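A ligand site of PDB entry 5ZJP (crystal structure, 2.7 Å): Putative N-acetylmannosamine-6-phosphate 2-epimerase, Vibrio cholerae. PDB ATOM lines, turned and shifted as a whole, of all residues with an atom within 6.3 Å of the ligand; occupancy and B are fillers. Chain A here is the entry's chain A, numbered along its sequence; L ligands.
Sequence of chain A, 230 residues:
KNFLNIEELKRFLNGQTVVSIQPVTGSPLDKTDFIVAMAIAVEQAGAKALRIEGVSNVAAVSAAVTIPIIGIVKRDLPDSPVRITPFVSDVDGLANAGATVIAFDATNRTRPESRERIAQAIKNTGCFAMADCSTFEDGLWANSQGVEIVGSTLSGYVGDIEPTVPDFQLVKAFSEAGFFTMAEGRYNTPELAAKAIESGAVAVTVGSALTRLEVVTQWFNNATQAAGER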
ATOM      1  N   SER A  20       4.049  27.598 -30.313  1.00  0.00           N
ATOM      2  CA  SER A  20       2.904  28.242 -29.676  1.00  0.00           C
ATOM      3  C   SER A  20       3.415  29.047 -28.498  1.00  0.00           C
ATOM      4  O   SER A  20       3.827  28.484 -27.475  1.00  0.00           O
ATOM      5  CB  SER A  20       1.869  27.206 -29.237  1.00  0.00           C
ATOM      6  OG  SER A  20       0.813  27.819 -28.523  1.00  0.00           O
ATOM      7  N   GLN A  22       2.442  31.004 -25.713  1.00  0.00           N
ATOM      8  CA  GLN A  22       1.335  31.334 -24.807  1.00  0.00           C
ATOM      9  C   GLN A  22       1.851  31.137 -23.386  1.00  0.00           C
ATOM     10  O   GLN A  22       1.695  30.063 -22.804  1.00  0.00           O
ATOM     11  CB  GLN A  22       0.113  30.465 -25.073  1.00  0.00           C
ATOM     12  CG  GLN A  22      -0.357  30.462 -26.518  1.00  0.00           C
ATOM     13  CD  GLN A  22      -1.641  29.688 -26.699  1.00  0.00           C
ATOM     14  OE1 GLN A  22      -2.281  29.278 -25.727  1.00  0.00           O
ATOM     15  NE2 GLN A  22      -2.017  29.463 -27.948  1.00  0.00           N
ATOM     16  N   ARG A  51       1.898  30.086 -33.107  1.00  0.00           N
ATOM     17  CA  ARG A  51       0.547  30.223 -32.570  1.00  0.00           C
ATOM     18  C   ARG A  51       0.582  31.286 -31.480  1.00  0.00           C
ATOM     19  O   ARG A  51       1.305  31.137 -30.486  1.00  0.00           O
ATOM     20  CB  ARG A  51       0.017  28.904 -32.026  1.00  0.00           C
ATOM     21  CG  ARG A  51      -1.354  29.016 -31.380  1.00  0.00           C
ATOM     22  CD  ARG A  51      -1.824  27.705 -30.784  1.00  0.00           C
ATOM     23  NE  ARG A  51      -2.415  26.807 -31.777  1.00  0.00           N
ATOM     24  CZ  ARG A  51      -3.709  26.520 -31.844  1.00  0.00           C
ATOM     25  NH1 ARG A  51      -4.560  27.066 -30.979  1.00  0.00           N
ATOM     26  NH2 ARG A  51      -4.172  25.701 -32.773  1.00  0.00           N
ATOM     27  N   ILE A  72      -5.548  33.004 -32.190  1.00  0.00           N
ATOM     28  CA  ILE A  72      -6.647  32.529 -31.365  1.00  0.00           C
ATOM     29  C   ILE A  72      -6.920  33.588 -30.305  1.00  0.00           C
ATOM     30  O   ILE A  72      -6.095  34.455 -30.035  1.00  0.00           O
ATOM     31  CB  ILE A  72      -6.376  31.175 -30.675  1.00  0.00           C
ATOM     32  CG1 ILE A  72      -5.215  31.282 -29.693  1.00  0.00           C
ATOM     33  CG2 ILE A  72      -6.130  30.067 -31.693  1.00  0.00           C
ATOM     34  CD1 ILE A  72      -5.068  30.082 -28.779  1.00  0.00           C
ATOM     35  N   LYS A  74      -8.519  33.262 -26.245  1.00  0.00           N
ATOM     36  CA  LYS A  74      -8.968  32.344 -25.204  1.00  0.00           C
ATOM     37  C   LYS A  74      -9.882  33.086 -24.252  1.00  0.00           C
ATOM     38  O   LYS A  74      -9.518  34.150 -23.730  1.00  0.00           O
ATOM     39  CB  LYS A  74      -7.793  31.748 -24.426  1.00  0.00           C
ATOM     40  CG  LYS A  74      -6.993  30.682 -25.144  1.00  0.00           C
ATOM     41  CD  LYS A  74      -6.137  29.917 -24.137  1.00  0.00           C
ATOM     42  CE  LYS A  74      -5.317  28.840 -24.815  1.00  0.00           C
ATOM     43  NZ  LYS A  74      -6.197  27.800 -25.410  1.00  0.00           N
ATOM     44  N   ARG A  83     -13.350  27.368 -25.106  1.00  0.00           N
ATOM     45  CA  ARG A  83     -12.415  28.432 -24.752  1.00  0.00           C
ATOM     46  C   ARG A  83     -11.728  29.072 -25.948  1.00  0.00           C
ATOM     47  O   ARG A  83     -11.476  30.282 -25.928  1.00  0.00           O
ATOM     48  CB  ARG A  83     -11.345  27.902 -23.787  1.00  0.00           C
ATOM     49  CG  ARG A  83     -11.915  27.394 -22.467  1.00  0.00           C
ATOM     50  CD  ARG A  83     -10.850  26.853 -21.523  1.00  0.00           C
ATOM     51  NE  ARG A  83     -10.017  27.902 -20.951  1.00  0.00           N
ATOM     52  CZ  ARG A  83      -8.698  28.003 -21.121  1.00  0.00           C
ATOM     53  NH1 ARG A  83      -8.060  27.111 -21.854  1.00  0.00           N
ATOM     54  NH2 ARG A  83      -8.030  28.992 -20.543  1.00  0.00           N
ATOM     55  N   ILE A  84     -11.403  28.311 -26.994  1.00  0.00           N
ATOM     56  CA  ILE A  84     -10.529  28.766 -28.065  1.00  0.00           C
ATOM     57  C   ILE A  84     -11.384  29.473 -29.117  1.00  0.00           C
ATOM     58  O   ILE A  84     -12.072  28.826 -29.912  1.00  0.00           O
ATOM     59  CB  ILE A  84      -9.735  27.604 -28.671  1.00  0.00           C
ATOM     60  CG1 ILE A  84      -8.736  27.062 -27.649  1.00  0.00           C
ATOM     61  CG2 ILE A  84      -9.001  28.060 -29.924  1.00  0.00           C
ATOM     62  CD1 ILE A  84      -8.144  25.715 -28.039  1.00  0.00           C
ATOM     63  N   ASP A 132      -9.731  23.148 -34.162  1.00  0.00           N
ATOM     64  CA  ASP A 132      -9.210  22.476 -32.975  1.00  0.00           C
ATOM     65  C   ASP A 132     -10.188  21.367 -32.618  1.00  0.00           C
ATOM     66  O   ASP A 132     -11.319  21.636 -32.191  1.00  0.00           O
ATOM     67  CB  ASP A 132      -9.044  23.463 -31.826  1.00  0.00           C
ATOM     68  CG  ASP A 132      -7.841  24.377 -32.004  1.00  0.00           C
ATOM     69  OD1 ASP A 132      -6.916  24.013 -32.763  1.00  0.00           O
ATOM     70  OD2 ASP A 132      -7.827  25.466 -31.390  1.00  0.00           O
ATOM     71  N   THR A 153      -5.657  19.298 -31.353  1.00  0.00           N
ATOM     72  CA  THR A 153      -5.419  20.192 -30.227  1.00  0.00           C
ATOM     73  C   THR A 153      -6.184  19.785 -28.970  1.00  0.00           C
ATOM     74  O   THR A 153      -5.626  19.795 -27.864  1.00  0.00           O
ATOM     75  CB  THR A 153      -5.791  21.622 -30.629  1.00  0.00           C
ATOM     76  OG1 THR A 153      -5.040  22.006 -31.784  1.00  0.00           O
ATOM     77  CG2 THR A 153      -5.484  22.602 -29.500  1.00  0.00           C
ATOM     78  N   LEU A 154      -7.456  19.432 -29.119  1.00  0.00           N
ATOM     79  CA  LEU A 154      -8.348  19.270 -27.973  1.00  0.00           C
ATOM     80  C   LEU A 154      -8.556  17.817 -27.564  1.00  0.00           C
ATOM     81  O   LEU A 154      -9.381  17.550 -26.675  1.00  0.00           O
ATOM     82  CB  LEU A 154      -9.697  19.915 -28.279  1.00  0.00           C
ATOM     83  CG  LEU A 154      -9.681  21.443 -28.384  1.00  0.00           C
ATOM     84  CD1 LEU A 154     -11.053  21.972 -28.744  1.00  0.00           C
ATOM     85  CD2 LEU A 154      -9.185  22.070 -27.085  1.00  0.00           C
ATOM     86  N   TYR A 157      -8.862  16.745 -23.676  1.00  0.00           N
ATOM     87  CA  TYR A 157      -9.166  17.920 -22.872  1.00  0.00           C
ATOM     88  C   TYR A 157     -10.664  18.172 -22.808  1.00  0.00           C
ATOM     89  O   TYR A 157     -11.107  19.308 -22.627  1.00  0.00           O
ATOM     90  CB  TYR A 157      -8.453  19.150 -23.425  1.00  0.00           C
ATOM     91  CG  TYR A 157      -6.943  19.045 -23.473  1.00  0.00           C
ATOM     92  CD1 TYR A 157      -6.221  18.647 -22.356  1.00  0.00           C
ATOM     93  CD2 TYR A 157      -6.247  19.341 -24.634  1.00  0.00           C
ATOM     94  CE1 TYR A 157      -4.839  18.553 -22.400  1.00  0.00           C
ATOM     95  CE2 TYR A 157      -4.867  19.239 -24.682  1.00  0.00           C
ATOM     96  CZ  TYR A 157      -4.166  18.847 -23.568  1.00  0.00           C
ATOM     97  OH  TYR A 157      -2.800  18.746 -23.614  1.00  0.00           O
ATOM     98  N   GLU A 184      -0.974  18.571 -32.526  1.00  0.00           N
ATOM     99  CA  GLU A 184      -0.871  19.495 -31.409  1.00  0.00           C
ATOM    100  C   GLU A 184      -1.378  18.810 -30.145  1.00  0.00           C
ATOM    101  O   GLU A 184      -2.418  18.159 -30.165  1.00  0.00           O
ATOM    102  CB  GLU A 184      -1.663  20.789 -31.681  1.00  0.00           C
ATOM    103  CG  GLU A 184      -1.597  21.806 -30.554  1.00  0.00           C
ATOM    104  CD  GLU A 184      -2.249  23.125 -30.915  1.00  0.00           C
ATOM    105  OE1 GLU A 184      -2.523  23.340 -32.117  1.00  0.00           O
ATOM    106  OE2 GLU A 184      -2.484  23.949 -30.016  1.00  0.00           O
ATOM    107  N   GLY A 185      -0.631  18.983 -29.058  1.00  0.00           N
ATOM    108  CA  GLY A 185      -1.011  18.394 -27.792  1.00  0.00           C
ATOM    109  C   GLY A 185      -0.014  17.396 -27.232  1.00  0.00           C
ATOM    110  O   GLY A 185       0.087  16.267 -27.736  1.00  0.00           O
ATOM    111  N   ARG A 186       0.735  17.815 -26.215  1.00  0.00           N
ATOM    112  CA  ARG A 186       1.593  16.967 -25.391  1.00  0.00           C
ATOM    113  C   ARG A 186       2.853  16.495 -26.107  1.00  0.00           C
ATOM    114  O   ARG A 186       3.492  15.550 -25.654  1.00  0.00           O
ATOM    115  CB  ARG A 186       0.838  15.756 -24.840  1.00  0.00           C
ATOM    116  CG  ARG A 186      -0.314  16.098 -23.915  1.00  0.00           C
ATOM    117  CD  ARG A 186      -0.988  14.836 -23.407  1.00  0.00           C
ATOM    118  NE  ARG A 186      -1.952  14.284 -24.362  1.00  0.00           N
ATOM    119  CZ  ARG A 186      -3.191  14.710 -24.511  1.00  0.00           C
ATOM    120  NH1 ARG A 186      -3.647  15.717 -23.765  1.00  0.00           N
ATOM    121  NH2 ARG A 186      -3.988  14.145 -25.412  1.00  0.00           N
ATOM    122  N   TYR A 187       3.228  17.123 -27.218  1.00  0.00           N
ATOM    123  CA  TYR A 187       4.480  16.783 -27.900  1.00  0.00           C
ATOM    124  C   TYR A 187       5.610  17.518 -27.190  1.00  0.00           C
ATOM    125  O   TYR A 187       6.012  18.618 -27.574  1.00  0.00           O
ATOM    126  CB  TYR A 187       4.418  17.121 -29.382  1.00  0.00           C
ATOM    127  CG  TYR A 187       3.445  16.268 -30.144  1.00  0.00           C
ATOM    128  CD1 TYR A 187       3.778  14.966 -30.521  1.00  0.00           C
ATOM    129  CD2 TYR A 187       2.189  16.741 -30.505  1.00  0.00           C
ATOM    130  CE1 TYR A 187       2.889  14.178 -31.220  1.00  0.00           C
ATOM    131  CE2 TYR A 187       1.299  15.959 -31.217  1.00  0.00           C
ATOM    132  CZ  TYR A 187       1.652  14.676 -31.572  1.00  0.00           C
ATOM    133  OH  TYR A 187       0.776  13.888 -32.273  1.00  0.00           O
ATOM    134  N   ASN A 188       6.129  16.882 -26.128  1.00  0.00           N
ATOM    135  CA  ASN A 188       6.973  17.560 -25.153  1.00  0.00           C
ATOM    136  C   ASN A 188       8.460  17.344 -25.388  1.00  0.00           C
ATOM    137  O   ASN A 188       9.272  17.956 -24.687  1.00  0.00           O
ATOM    138  CB  ASN A 188       6.609  17.083 -23.746  1.00  0.00           C
ATOM    139  CG  ASN A 188       5.214  17.503 -23.318  1.00  0.00           C
ATOM    140  OD1 ASN A 188       4.659  18.465 -23.843  1.00  0.00           O
ATOM    141  ND2 ASN A 188       4.639  16.770 -22.378  1.00  0.00           N
ATOM    142  N   THR A 205       2.656  21.444 -33.519  1.00  0.00           N
ATOM    143  CA  THR A 205       2.652  22.620 -32.653  1.00  0.00           C
ATOM    144  C   THR A 205       3.138  22.220 -31.266  1.00  0.00           C
ATOM    145  O   THR A 205       2.671  21.228 -30.703  1.00  0.00           O
ATOM    146  CB  THR A 205       1.255  23.232 -32.582  1.00  0.00           C
ATOM    147  OG1 THR A 205       0.834  23.637 -33.888  1.00  0.00           O
ATOM    148  CG2 THR A 205       1.256  24.454 -31.672  1.00  0.00           C
ATOM    149  N   VAL A 206       4.061  23.013 -30.711  1.00  0.00           N
ATOM    150  CA  VAL A 206       4.625  22.767 -29.398  1.00  0.00           C
ATOM    151  C   VAL A 206       4.564  24.069 -28.607  1.00  0.00           C
ATOM    152  O   VAL A 206       5.045  25.105 -29.079  1.00  0.00           O
ATOM    153  CB  VAL A 206       6.074  22.250 -29.476  1.00  0.00           C
ATOM    154  CG1 VAL A 206       6.656  22.042 -28.083  1.00  0.00           C
ATOM    155  CG2 VAL A 206       6.133  20.955 -30.279  1.00  0.00           C
ATOM    156  N   GLY A 207       3.989  24.010 -27.407  1.00  0.00           N
ATOM    157  CA  GLY A 207       3.818  25.200 -26.596  1.00  0.00           C
ATOM    158  C   GLY A 207       4.483  25.137 -25.236  1.00  0.00           C
ATOM    159  O   GLY A 207       5.437  25.882 -24.977  1.00  0.00           O
ATOM    160  N   SER A 208       3.976  24.274 -24.360  1.00  0.00           N
ATOM    161  CA  SER A 208       4.428  24.249 -22.966  1.00  0.00           C
ATOM    162  C   SER A 208       5.923  23.936 -22.877  1.00  0.00           C
ATOM    163  O   SER A 208       6.660  24.601 -22.141  1.00  0.00           O
ATOM    164  CB  SER A 208       3.622  23.235 -22.169  1.00  0.00           C
ATOM    165  OG  SER A 208       2.256  23.604 -22.095  1.00  0.00           O
ATOM    166  N   ALA A 209       6.380  22.922 -23.610  1.00  0.00           N
ATOM    167  CA  ALA A 209       7.777  22.529 -23.573  1.00  0.00           C
ATOM    168  C   ALA A 209       8.720  23.639 -24.013  1.00  0.00           C
ATOM    169  O   ALA A 209       9.921  23.564 -23.734  1.00  0.00           O
ATOM    170  CB  ALA A 209       7.999  21.282 -24.427  1.00  0.00           C
ATOM    171  N   LEU A 210       8.213  24.650 -24.709  1.00  0.00           N
ATOM    172  CA  LEU A 210       9.040  25.731 -25.253  1.00  0.00           C
ATOM    173  C   LEU A 210       8.837  27.076 -24.568  1.00  0.00           C
ATOM    174  O   LEU A 210       9.821  27.773 -24.312  1.00  0.00           O
ATOM    175  CB  LEU A 210       8.782  25.892 -26.753  1.00  0.00           C
ATOM    176  CG  LEU A 210       9.429  24.880 -27.689  1.00  0.00           C
ATOM    177  CD1 LEU A 210       8.902  25.033 -29.106  1.00  0.00           C
ATOM    178  CD2 LEU A 210      10.939  25.060 -27.676  1.00  0.00           C
ATOM    179  N   ARG A 212       6.577  27.886 -21.695  1.00  0.00           N
ATOM    180  CA  ARG A 212       5.987  27.933 -20.353  1.00  0.00           C
ATOM    181  C   ARG A 212       7.059  27.540 -19.345  1.00  0.00           C
ATOM    182  O   ARG A 212       7.216  26.357 -19.019  1.00  0.00           O
ATOM    183  CB  ARG A 212       4.753  27.038 -20.250  1.00  0.00           C
ATOM    184  CG  ARG A 212       3.519  27.633 -20.903  1.00  0.00           C
ATOM    185  CD  ARG A 212       2.344  26.673 -20.878  1.00  0.00           C
ATOM    186  NE  ARG A 212       1.135  27.271 -21.430  1.00  0.00           N
ATOM    187  CZ  ARG A 212       0.106  26.591 -21.917  1.00  0.00           C
ATOM    188  NH1 ARG A 212       0.132  25.262 -21.917  1.00  0.00           N
ATOM    189  NH2 ARG A 212      -0.950  27.217 -22.401  1.00  0.00           N
HETATM  190  P1  LIG L   1       1.481  21.924 -25.575  1.00  0.00           P
HETATM  191  C1  LIG L   1      -4.507  25.840 -27.081  1.00  0.00           C
HETATM  192  O1  LIG L   1      -3.967  26.520 -27.893  1.00  0.00           O
HETATM  193  C2  LIG L   1      -3.712  24.745 -26.372  1.00  0.00           C
HETATM  194  N1  LIG L   1      -4.527  23.811 -25.598  1.00  0.00           N
HETATM  195  C3  LIG L   1      -2.592  25.354 -25.509  1.00  0.00           C
HETATM  196  O2  LIG L   1      -2.934  25.280 -24.160  1.00  0.00           O
HETATM  197  C4  LIG L   1      -1.252  24.621 -25.705  1.00  0.00           C
HETATM  198  O3  LIG L   1      -0.220  25.540 -25.488  1.00  0.00           O
HETATM  199  C5  LIG L   1      -1.063  24.005 -27.099  1.00  0.00           C
HETATM  200  O4  LIG L   1      -1.734  22.789 -27.241  1.00  0.00           O
HETATM  201  C6  LIG L   1       0.418  23.654 -27.234  1.00  0.00           C
HETATM  202  O5  LIG L   1       0.528  22.312 -26.861  1.00  0.00           O
HETATM  203  C7  LIG L   1      -5.687  24.166 -24.769  1.00  0.00           C
HETATM  204  O6  LIG L   1      -6.057  25.284 -24.652  1.00  0.00           O
HETATM  205  C8  LIG L   1      -6.420  23.056 -24.036  1.00  0.00           C
HETATM  206  O7  LIG L   1       2.902  21.731 -26.045  1.00  0.00           O
HETATM  207  O8  LIG L   1       0.979  20.648 -24.943  1.00  0.00           O
HETATM  208  O9  LIG L   1       1.423  23.041 -24.559  1.00  0.00           O
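The side-chain amino group (NZ) of Lys 74 is in hydrogen-bond range of an oxygen (O6) of the ligand. The backbone NH (N) of Ser 208 sits at hydrogen-bond distance from an oxygen (O9) of the ligand, 2.8 Å away. The side-chain hydroxyl (OG) of Ser 208 sits at hydrogen-bond distance from an oxygen (O9) of the ligand. The backbone NH (N) of Gly 207 lies within hydrogen-bond range of an oxygen (O7) of the ligand. O4 of the ligand is in hydrogen-bond range of OE2 of Glu 184, at 3.1 Å. An oxygen (O8) of the ligand sits at hydrogen-bond distance from the backbone NH (N) of Arg 186. An oxygen (O1) of the ligand lies within hydrogen-bond range of the guanidinium group of Arg 51, 3.2 Å away. NH1 of Arg 212 is in salt-bridge range of O9 of the ligand (3.7 Å).
Residues that only touch the ligand: Gln 22, Ile 84, Tyr 157, Ile 72, Val 206, Arg 83 and Ser 20. Of the 23 residues printed, 14 come within 4 Å of the ligand. The nearest printed residue that does not touch the ligand is Gly 185 (4.1 Å).
The guanidinium group (NH1) of Arg 212 sits at hydrogen-bond distance from the side-chain hydroxyl (OG) of Ser 208 (2.7 Å). The side-chain carboxylate of Glu 184 is in salt-bridge range of the guanidinium group of Arg 51 (3.0 Å). The side-chain carboxylate (OE1) of Glu 184 is in hydrogen-bond range of the side-chain hydroxyl (OG1) of Thr 153 (2.9 Å). NH1 of Arg 186 is in hydrogen-bond range of OH of Tyr 157, 3.1 Å away. OD1 of Asp 132 lies within salt-bridge range of NH2 of Arg 51 (3.2 Å). O of Gln 22 lies within hydrogen-bond range of NE of Arg 212, at 3.2 Å. OG of Ser 20 sits at hydrogen-bond distance from NE2 of Gln 22. The backbone NH of Ser 20 sits at hydrogen-bond distance from the backbone carbonyl oxygen of Val 206 (3.0 Å).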
